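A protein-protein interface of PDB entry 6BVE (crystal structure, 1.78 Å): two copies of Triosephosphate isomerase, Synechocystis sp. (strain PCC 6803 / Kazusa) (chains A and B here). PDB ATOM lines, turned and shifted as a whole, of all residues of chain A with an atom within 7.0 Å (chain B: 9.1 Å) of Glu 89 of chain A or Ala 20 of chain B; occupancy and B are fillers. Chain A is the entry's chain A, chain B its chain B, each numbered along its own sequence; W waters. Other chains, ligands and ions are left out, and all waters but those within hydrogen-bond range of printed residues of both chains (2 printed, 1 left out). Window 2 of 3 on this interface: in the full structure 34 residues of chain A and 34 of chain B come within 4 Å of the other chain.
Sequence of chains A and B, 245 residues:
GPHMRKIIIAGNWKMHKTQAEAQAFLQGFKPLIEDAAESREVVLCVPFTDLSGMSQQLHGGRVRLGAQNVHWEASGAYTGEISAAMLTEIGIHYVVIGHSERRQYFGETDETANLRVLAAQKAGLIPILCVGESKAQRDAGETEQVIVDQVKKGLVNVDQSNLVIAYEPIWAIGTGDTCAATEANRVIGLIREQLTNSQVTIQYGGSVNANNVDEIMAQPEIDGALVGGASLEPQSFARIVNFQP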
ATOM      1  N   SER A  52      21.256  -7.635  17.114  1.00  0.00           N
ATOM      2  CA  SER A  52      20.342  -6.526  16.840  1.00  0.00           C
ATOM      3  C   SER A  52      19.562  -6.135  18.088  1.00  0.00           C
ATOM      4  O   SER A  52      19.473  -4.950  18.435  1.00  0.00           O
ATOM      5  CB  SER A  52      19.382  -6.901  15.708  1.00  0.00           C
ATOM      6  OG  SER A  52      20.047  -6.915  14.464  1.00  0.00           O
ATOM      7  N   SER A  55      21.823  -4.511  20.554  1.00  0.00           N
ATOM      8  CA  SER A  55      22.177  -3.194  20.038  1.00  0.00           C
ATOM      9  C   SER A  55      21.154  -2.142  20.458  1.00  0.00           C
ATOM     10  O   SER A  55      21.518  -1.039  20.891  1.00  0.00           O
ATOM     11  CB  SER A  55      22.294  -3.252  18.515  1.00  0.00           C
ATOM     12  OG  SER A  55      23.052  -2.167  18.015  1.00  0.00           O
ATOM     13  N   ALA A  84      30.888  -8.720   6.843  1.00  0.00           N
ATOM     14  CA  ALA A  84      31.138  -7.479   7.573  1.00  0.00           C
ATOM     15  C   ALA A  84      29.990  -6.484   7.404  1.00  0.00           C
ATOM     16  O   ALA A  84      29.624  -5.786   8.360  1.00  0.00           O
ATOM     17  CB  ALA A  84      32.454  -6.861   7.101  1.00  0.00           C
ATOM     18  N   ALA A  85      29.425  -6.393   6.194  1.00  0.00           N
ATOM     19  CA  ALA A  85      28.322  -5.462   5.944  1.00  0.00           C
ATOM     20  C   ALA A  85      27.102  -5.801   6.789  1.00  0.00           C
ATOM     21  O   ALA A  85      26.375  -4.908   7.246  1.00  0.00           O
ATOM     22  CB  ALA A  85      27.950  -5.463   4.461  1.00  0.00           C
ATOM     23  N   MET A  86      26.852  -7.094   7.003  1.00  0.00           N
ATOM     24  CA  MET A  86      25.762  -7.488   7.892  1.00  0.00           C
ATOM     25  C   MET A  86      26.012  -7.021   9.315  1.00  0.00           C
ATOM     26  O   MET A  86      25.065  -6.656  10.031  1.00  0.00           O
ATOM     27  CB  MET A  86      25.584  -9.001   7.852  1.00  0.00           C
ATOM     28  CG  MET A  86      25.132  -9.486   6.469  1.00  0.00           C
ATOM     29  SD  MET A  86      25.221 -11.281   6.329  1.00  0.00           S
ATOM     30  CE  MET A  86      25.017 -11.462   4.551  1.00  0.00           C
ATOM     31  N   LEU A  87      27.276  -7.005   9.738  1.00  0.00           N
ATOM     32  CA  LEU A  87      27.586  -6.581  11.099  1.00  0.00           C
ATOM     33  C   LEU A  87      27.578  -5.064  11.247  1.00  0.00           C
ATOM     34  O   LEU A  87      27.073  -4.537  12.251  1.00  0.00           O
ATOM     35  CB  LEU A  87      28.944  -7.151  11.515  1.00  0.00           C
ATOM     36  CG  LEU A  87      29.017  -8.681  11.603  1.00  0.00           C
ATOM     37  CD1 LEU A  87      30.390  -9.142  12.110  1.00  0.00           C
ATOM     38  CD2 LEU A  87      27.908  -9.233  12.510  1.00  0.00           C
ATOM     39  N   THR A  88      28.153  -4.336  10.286  1.00  0.00           N
ATOM     40  CA  THR A  88      28.180  -2.890  10.446  1.00  0.00           C
ATOM     41  C   THR A  88      26.790  -2.292  10.308  1.00  0.00           C
ATOM     42  O   THR A  88      26.534  -1.215  10.860  1.00  0.00           O
ATOM     43  CB  THR A  88      29.139  -2.232   9.443  1.00  0.00           C
ATOM     44  OG1 THR A  88      28.686  -2.472   8.119  1.00  0.00           O
ATOM     45  CG2 THR A  88      30.544  -2.770   9.592  1.00  0.00           C
ATOM     46  N   GLU A  89      25.881  -2.962   9.600  1.00  0.00           N
ATOM     47  CA  GLU A  89      24.514  -2.455   9.526  1.00  0.00           C
ATOM     48  C   GLU A  89      23.894  -2.364  10.920  1.00  0.00           C
ATOM     49  O   GLU A  89      23.144  -1.417  11.216  1.00  0.00           O
ATOM     50  CB  GLU A  89      23.665  -3.342   8.611  1.00  0.00           C
ATOM     51  CG  GLU A  89      22.217  -2.891   8.506  1.00  0.00           C
ATOM     52  CD  GLU A  89      21.380  -3.826   7.658  1.00  0.00           C
ATOM     53  OE1 GLU A  89      21.510  -5.053   7.847  1.00  0.00           O
ATOM     54  OE2 GLU A  89      20.612  -3.341   6.805  1.00  0.00           O
ATOM     55  N   ILE A  90      24.228  -3.323  11.795  1.00  0.00           N
ATOM     56  CA  ILE A  90      23.730  -3.339  13.167  1.00  0.00           C
ATOM     57  C   ILE A  90      24.435  -2.292  14.015  1.00  0.00           C
ATOM     58  O   ILE A  90      23.876  -1.831  15.014  1.00  0.00           O
ATOM     59  CB  ILE A  90      23.896  -4.743  13.785  1.00  0.00           C
ATOM     60  CG1 ILE A  90      23.256  -5.788  12.862  1.00  0.00           C
ATOM     61  CG2 ILE A  90      23.326  -4.813  15.233  1.00  0.00           C
ATOM     62  CD1 ILE A  90      23.537  -7.260  13.250  1.00  0.00           C
ATOM     63  N   GLY A  91      25.639  -1.889  13.638  1.00  0.00           N
ATOM     64  CA  GLY A  91      26.342  -0.871  14.381  1.00  0.00           C
ATOM     65  C   GLY A  91      27.245  -1.403  15.464  1.00  0.00           C
ATOM     66  O   GLY A  91      27.636  -0.641  16.358  1.00  0.00           O
ATOM     67  N   ILE A  92      27.617  -2.677  15.403  1.00  0.00           N
ATOM     68  CA  ILE A  92      28.449  -3.229  16.464  1.00  0.00           C
ATOM     69  C   ILE A  92      29.891  -2.797  16.251  1.00  0.00           C
ATOM     70  O   ILE A  92      30.251  -2.301  15.177  1.00  0.00           O
ATOM     71  CB  ILE A  92      28.320  -4.758  16.526  1.00  0.00           C
ATOM     72  CG1 ILE A  92      29.003  -5.395  15.325  1.00  0.00           C
ATOM     73  CG2 ILE A  92      26.843  -5.153  16.615  1.00  0.00           C
ATOM     74  CD1 ILE A  92      29.268  -6.879  15.509  1.00  0.00           C
ATOM     75  N   TRP B  13      20.076 -18.079   0.095  1.00  0.00           N
ATOM     76  CA  TRP B  13      20.767 -16.829  -0.216  1.00  0.00           C
ATOM     77  C   TRP B  13      22.258 -16.898   0.052  1.00  0.00           C
ATOM     78  O   TRP B  13      22.986 -16.008  -0.403  1.00  0.00           O
ATOM     79  CB  TRP B  13      20.191 -15.688   0.621  1.00  0.00           C
ATOM     80  CG  TRP B  13      18.909 -15.175   0.122  1.00  0.00           C
ATOM     81  CD1 TRP B  13      18.250 -15.553  -1.010  1.00  0.00           C
ATOM     82  CD2 TRP B  13      18.094 -14.189   0.763  1.00  0.00           C
ATOM     83  NE1 TRP B  13      17.061 -14.852  -1.120  1.00  0.00           N
ATOM     84  CE2 TRP B  13      16.954 -14.001  -0.047  1.00  0.00           C
ATOM     85  CE3 TRP B  13      18.224 -13.434   1.945  1.00  0.00           C
ATOM     86  CZ2 TRP B  13      15.943 -13.093   0.282  1.00  0.00           C
ATOM     87  CZ3 TRP B  13      17.206 -12.519   2.273  1.00  0.00           C
ATOM     88  CH2 TRP B  13      16.082 -12.371   1.451  1.00  0.00           C
ATOM     89  N   LYS B  17      22.792 -10.408   1.482  1.00  0.00           N
ATOM     90  CA  LYS B  17      21.686  -9.535   1.878  1.00  0.00           C
ATOM     91  C   LYS B  17      21.778  -9.082   3.336  1.00  0.00           C
ATOM     92  O   LYS B  17      21.626  -9.874   4.277  1.00  0.00           O
ATOM     93  CB  LYS B  17      20.324 -10.185   1.586  1.00  0.00           C
ATOM     94  CG  LYS B  17      20.124 -10.456   0.084  1.00  0.00           C
ATOM     95  CD  LYS B  17      18.659 -10.557  -0.273  1.00  0.00           C
ATOM     96  CE  LYS B  17      18.483 -11.041  -1.708  1.00  0.00           C
ATOM     97  NZ  LYS B  17      19.138 -10.106  -2.695  1.00  0.00           N
ATOM     98  N   THR B  18      22.054  -7.793   3.509  1.00  0.00           N
ATOM     99  CA  THR B  18      21.802  -7.115   4.770  1.00  0.00           C
ATOM    100  C   THR B  18      20.300  -7.128   5.068  1.00  0.00           C
ATOM    101  O   THR B  18      19.483  -7.526   4.243  1.00  0.00           O
ATOM    102  CB  THR B  18      22.292  -5.672   4.686  1.00  0.00           C
ATOM    103  OG1 THR B  18      21.530  -5.000   3.687  1.00  0.00           O
ATOM    104  CG2 THR B  18      23.779  -5.621   4.321  1.00  0.00           C
ATOM    105  N   GLN B  19      19.931  -6.640   6.258  1.00  0.00           N
ATOM    106  CA  GLN B  19      18.512  -6.528   6.578  1.00  0.00           C
ATOM    107  C   GLN B  19      17.801  -5.593   5.594  1.00  0.00           C
ATOM    108  O   GLN B  19      16.691  -5.886   5.132  1.00  0.00           O
ATOM    109  CB  GLN B  19      18.348  -6.041   8.018  1.00  0.00           C
ATOM    110  CG  GLN B  19      18.964  -7.012   9.035  1.00  0.00           C
ATOM    111  CD  GLN B  19      18.854  -6.511  10.464  1.00  0.00           C
ATOM    112  OE1 GLN B  19      19.841  -6.476  11.203  1.00  0.00           O
ATOM    113  NE2 GLN B  19      17.658  -6.111  10.854  1.00  0.00           N
ATOM    114  N   ALA B  20      18.453  -4.497   5.213  1.00  0.00           N
ATOM    115  CA  ALA B  20      17.843  -3.588   4.239  1.00  0.00           C
ATOM    116  C   ALA B  20      17.630  -4.280   2.891  1.00  0.00           C
ATOM    117  O   ALA B  20      16.569  -4.142   2.264  1.00  0.00           O
ATOM    118  CB  ALA B  20      18.720  -2.345   4.086  1.00  0.00           C
ATOM    119  N   GLU B  21      18.624  -5.039   2.433  1.00  0.00           N
ATOM    120  CA  GLU B  21      18.487  -5.745   1.164  1.00  0.00           C
ATOM    121  C   GLU B  21      17.446  -6.854   1.262  1.00  0.00           C
ATOM    122  O   GLU B  21      16.712  -7.124   0.300  1.00  0.00           O
ATOM    123  CB  GLU B  21      19.842  -6.294   0.742  1.00  0.00           C
ATOM    124  CG  GLU B  21      20.841  -5.190   0.442  1.00  0.00           C
ATOM    125  CD  GLU B  21      22.233  -5.709   0.203  1.00  0.00           C
ATOM    126  OE1 GLU B  21      22.629  -6.702   0.835  1.00  0.00           O
ATOM    127  OE2 GLU B  21      22.944  -5.111  -0.625  1.00  0.00           O
ATOM    128  N   ALA B  22      17.388  -7.531   2.403  1.00  0.00           N
ATOM    129  CA  ALA B  22      16.367  -8.559   2.575  1.00  0.00           C
ATOM    130  C   ALA B  22      14.964  -7.960   2.550  1.00  0.00           C
ATOM    131  O   ALA B  22      14.045  -8.536   1.959  1.00  0.00           O
ATOM    132  CB  ALA B  22      16.612  -9.318   3.883  1.00  0.00           C
ATOM    133  N   GLN B  23      14.785  -6.797   3.184  1.00  0.00           N
ATOM    134  CA  GLN B  23      13.491  -6.125   3.172  1.00  0.00           C
ATOM    135  C   GLN B  23      13.078  -5.746   1.751  1.00  0.00           C
ATOM    136  O   GLN B  23      11.924  -5.937   1.354  1.00  0.00           O
ATOM    137  CB  GLN B  23      13.574  -4.882   4.065  1.00  0.00           C
ATOM    138  CG  GLN B  23      12.262  -4.226   4.431  1.00  0.00           C
ATOM    139  CD  GLN B  23      11.617  -3.454   3.281  1.00  0.00           C
ATOM    140  OE1 GLN B  23      10.392  -3.475   3.141  1.00  0.00           O
ATOM    141  NE2 GLN B  23      12.430  -2.787   2.451  1.00  0.00           N
ATOM    142  N   ALA B  24      14.017  -5.213   0.977  1.00  0.00           N
ATOM    143  CA  ALA B  24      13.732  -4.829  -0.404  1.00  0.00           C
ATOM    144  C   ALA B  24      13.364  -6.047  -1.249  1.00  0.00           C
ATOM    145  O   ALA B  24      12.437  -5.991  -2.072  1.00  0.00           O
ATOM    146  CB  ALA B  24      14.943  -4.107  -0.990  1.00  0.00           C
ATOM    147  N   PHE B  25      14.058  -7.166  -1.038  1.00  0.00           N
ATOM    148  CA  PHE B  25      13.683  -8.404  -1.718  1.00  0.00           C
ATOM    149  C   PHE B  25      12.237  -8.768  -1.420  1.00  0.00           C
ATOM    150  O   PHE B  25      11.459  -9.059  -2.333  1.00  0.00           O
ATOM    151  CB  PHE B  25      14.634  -9.536  -1.319  1.00  0.00           C
ATOM    152  CG  PHE B  25      14.278 -10.886  -1.940  1.00  0.00           C
ATOM    153  CD1 PHE B  25      13.258 -11.677  -1.404  1.00  0.00           C
ATOM    154  CD2 PHE B  25      14.976 -11.354  -3.037  1.00  0.00           C
ATOM    155  CE1 PHE B  25      12.938 -12.914  -1.960  1.00  0.00           C
ATOM    156  CE2 PHE B  25      14.657 -12.603  -3.612  1.00  0.00           C
ATOM    157  CZ  PHE B  25      13.637 -13.374  -3.072  1.00  0.00           C
ATOM    158  N   LEU B  26      11.847  -8.754  -0.141  1.00  0.00           N
ATOM    159  CA  LEU B  26      10.489  -9.179   0.193  1.00  0.00           C
ATOM    160  C   LEU B  26       9.440  -8.275  -0.430  1.00  0.00           C
ATOM    161  O   LEU B  26       8.368  -8.756  -0.808  1.00  0.00           O
ATOM    162  CB  LEU B  26      10.286  -9.227   1.705  1.00  0.00           C
ATOM    163  CG  LEU B  26      11.001 -10.377   2.396  1.00  0.00           C
ATOM    164  CD1 LEU B  26      10.671 -10.303   3.884  1.00  0.00           C
ATOM    165  CD2 LEU B  26      10.577 -11.712   1.796  1.00  0.00           C
ATOM    166  N   GLN B  27       9.739  -6.971  -0.553  1.00  0.00           N
ATOM    167  CA  GLN B  27       8.822  -6.044  -1.209  1.00  0.00           C
ATOM    168  C   GLN B  27       8.541  -6.466  -2.634  1.00  0.00           C
ATOM    169  O   GLN B  27       7.394  -6.402  -3.092  1.00  0.00           O
ATOM    170  CB  GLN B  27       9.396  -4.623  -1.215  1.00  0.00           C
ATOM    171  CG  GLN B  27       9.522  -4.003   0.132  1.00  0.00           C
ATOM    172  CD  GLN B  27       8.181  -3.684   0.745  1.00  0.00           C
ATOM    173  OE1 GLN B  27       7.156  -3.717   0.065  1.00  0.00           O
ATOM    174  NE2 GLN B  27       8.175  -3.365   2.040  1.00  0.00           N
ATOM    175  N   PRO B  47      20.701 -15.363   5.969  1.00  0.00           N
ATOM    176  CA  PRO B  47      21.722 -15.203   7.014  1.00  0.00           C
ATOM    177  C   PRO B  47      21.095 -15.042   8.389  1.00  0.00           C
ATOM    178  O   PRO B  47      19.980 -14.537   8.521  1.00  0.00           O
ATOM    179  CB  PRO B  47      22.462 -13.929   6.601  1.00  0.00           C
ATOM    180  CG  PRO B  47      22.284 -13.877   5.071  1.00  0.00           C
ATOM    181  CD  PRO B  47      20.920 -14.451   4.818  1.00  0.00           C
ATOM    182  N   THR B  49      21.539 -12.959  10.687  1.00  0.00           N
ATOM    183  CA  THR B  49      21.234 -11.577  11.046  1.00  0.00           C
ATOM    184  C   THR B  49      20.000 -11.025  10.334  1.00  0.00           C
ATOM    185  O   THR B  49      19.539  -9.927  10.681  1.00  0.00           O
ATOM    186  CB  THR B  49      22.464 -10.724  10.752  1.00  0.00           C
ATOM    187  OG1 THR B  49      22.970 -11.066   9.461  1.00  0.00           O
ATOM    188  CG2 THR B  49      23.560 -11.011  11.783  1.00  0.00           C
ATOM    189  N   ASP B  50      19.440 -11.758   9.370  1.00  0.00           N
ATOM    190  CA  ASP B  50      18.209 -11.363   8.696  1.00  0.00           C
ATOM    191  C   ASP B  50      16.969 -12.061   9.244  1.00  0.00           C
ATOM    192  O   ASP B  50      15.853 -11.687   8.867  1.00  0.00           O
ATOM    193  CB  ASP B  50      18.279 -11.677   7.197  1.00  0.00           C
ATOM    194  CG  ASP B  50      19.295 -10.816   6.446  1.00  0.00           C
ATOM    195  OD1 ASP B  50      19.619  -9.715   6.924  1.00  0.00           O
ATOM    196  OD2 ASP B  50      19.761 -11.255   5.374  1.00  0.00           O
ATOM    197  N   GLY B  53      14.300  -9.910  11.598  1.00  0.00           N
ATOM    198  CA  GLY B  53      13.658  -8.831  10.846  1.00  0.00           C
ATOM    199  C   GLY B  53      12.716  -9.333   9.767  1.00  0.00           C
ATOM    200  O   GLY B  53      11.625  -8.791   9.577  1.00  0.00           O
ATOM    201  N   MET B  54      13.126 -10.368   9.033  1.00  0.00           N
ATOM    202  CA  MET B  54      12.243 -10.928   8.018  1.00  0.00           C
ATOM    203  C   MET B  54      11.041 -11.607   8.645  1.00  0.00           C
ATOM    204  O   MET B  54       9.943 -11.569   8.083  1.00  0.00           O
ATOM    205  CB  MET B  54      13.003 -11.925   7.144  1.00  0.00           C
ATOM    206  CG  MET B  54      14.099 -11.273   6.348  1.00  0.00           C
ATOM    207  SD  MET B  54      14.947 -12.439   5.262  1.00  0.00           S
ATOM    208  CE  MET B  54      13.658 -12.775   4.068  1.00  0.00           C
ATOM    209  N   GLN B  57       8.249  -9.336   9.061  1.00  0.00           N
ATOM    210  CA  GLN B  57       7.616  -8.938   7.808  1.00  0.00           C
ATOM    211  C   GLN B  57       6.804 -10.061   7.175  1.00  0.00           C
ATOM    212  O   GLN B  57       6.135  -9.827   6.163  1.00  0.00           O
ATOM    213  CB  GLN B  57       8.670  -8.455   6.802  1.00  0.00           C
ATOM    214  CG  GLN B  57       9.650  -7.417   7.334  1.00  0.00           C
ATOM    215  CD  GLN B  57      10.854  -7.220   6.412  1.00  0.00           C
ATOM    216  OE1 GLN B  57      10.697  -6.882   5.238  1.00  0.00           O
ATOM    217  NE2 GLN B  57      12.060  -7.440   6.940  1.00  0.00           N
HETATM  218  O   HOH W   1      19.874  -4.413  13.611  1.00  0.00           O
HETATM  219  O   HOH W   2      20.244  -9.066  13.098  1.00  0.00           O
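Printed residues of chain A that touch a printed residue of chain B: Ser 52, Ala 85, Met 86, Glu 89 and Ile 90. Hydrophobic or aromatic side chains of chain A within 4 Å of the printed part of chain B: Met 86 and Ile 90. Along chain A the printed residues that touch a printed residue of chain B span positions 52 to 90. Among the printed residues, 9 pairs touch across the chains. Among the printed residues, no Asp or Glu carboxylate lies within 4 Å of a Lys or Arg side-chain nitrogen of the other chain.
Water W2 lies within hydrogen-bond range of OG of Ser 52 of chain A, O of Thr 49 of chain B and OE1 of Gln 19 of chain B. Water W1 lies within hydrogen-bond range of OG of Ser 52 of chain A (2.6 Å) and OE1 of Gln 19 of chain B (3.2 Å).
Among the printed residues, merely in contact across the chains: Ala 85 of chain A with Thr 18 of chain B, Met 86 of chain A with Lys 17 of chain B, Met 86 of chain A with Pro 47 of chain B, Met 86 of chain A with Thr 49 of chain B, Glu 89 of chain A with Thr 18 of chain B and Ile 90 of chain A with Gln 19 of chain B.
No position is printed for both chains.
Printed residues of chain B within 4 Å of Ala 85 of chain A: Thr 18 (3.98 Å). Printed residues of chain B within 4 Å of Met 86 of chain A: Lys 17, Pro 47 and Thr 49. Leu 87 of chain A touches none of the printed residues of chain B. No residue of chain B comes within 4 Å of Thr 88 of chain A. Of chain B, only Thr 18 (3.3 Å), Gln 19 (2.7 Å) and Ala 20 (2.9 Å) come within 4 Å of Glu 89 of chain A. Ala 20 of chain B touches one residue of chain A. Gln 23 of chain B touches none of the printed residues of chain A. Of the printed residues of chain A, Thr 49 of chain B touches Met 86 (3.7 Å).
The side-chain hydroxyl (OG) of Ser 55 of chain A lies within hydrogen-bond range of the backbone carbonyl oxygen (O) of Ile 90 of chain A (3.1 Å). The side-chain hydroxyl (OG1) of Thr 88 of chain A lies within hydrogen-bond range of the backbone carbonyl oxygen (O) of Ala 85 of chain A. O of Lys 17 of chain B lies close to OD2 of Asp 50 of chain B, at 2.6 Å. The side-chain hydroxyl (OG1) of Thr 18 of chain B lies close to the backbone NH (N) of Ala 20 of chain B (3.5 Å). OE1 of Glu 21 of chain B is in hydrogen-bond range of N of Thr 18 of chain B (2.9 Å). The backbone NH (N) of Gln 19 of chain B is in hydrogen-bond range of the side-chain carboxylate (OD1) of Asp 50 of chain B, 3.2 Å away.
The side-chain hydroxyl of Ser 52 of chain A lies within hydrogen-bond range of the side-chain amide oxygen of Gln 19 of chain B (3.3 Å). OE1 of Glu 89 of chain A sits at hydrogen-bond distance from N of Gln 19 of chain B (2.7 Å). The backbone NH (N) of Ala 20 of chain B sits at hydrogen-bond distance from the side-chain carboxylate (OE2) of Glu 89 of chain A (2.9 Å).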
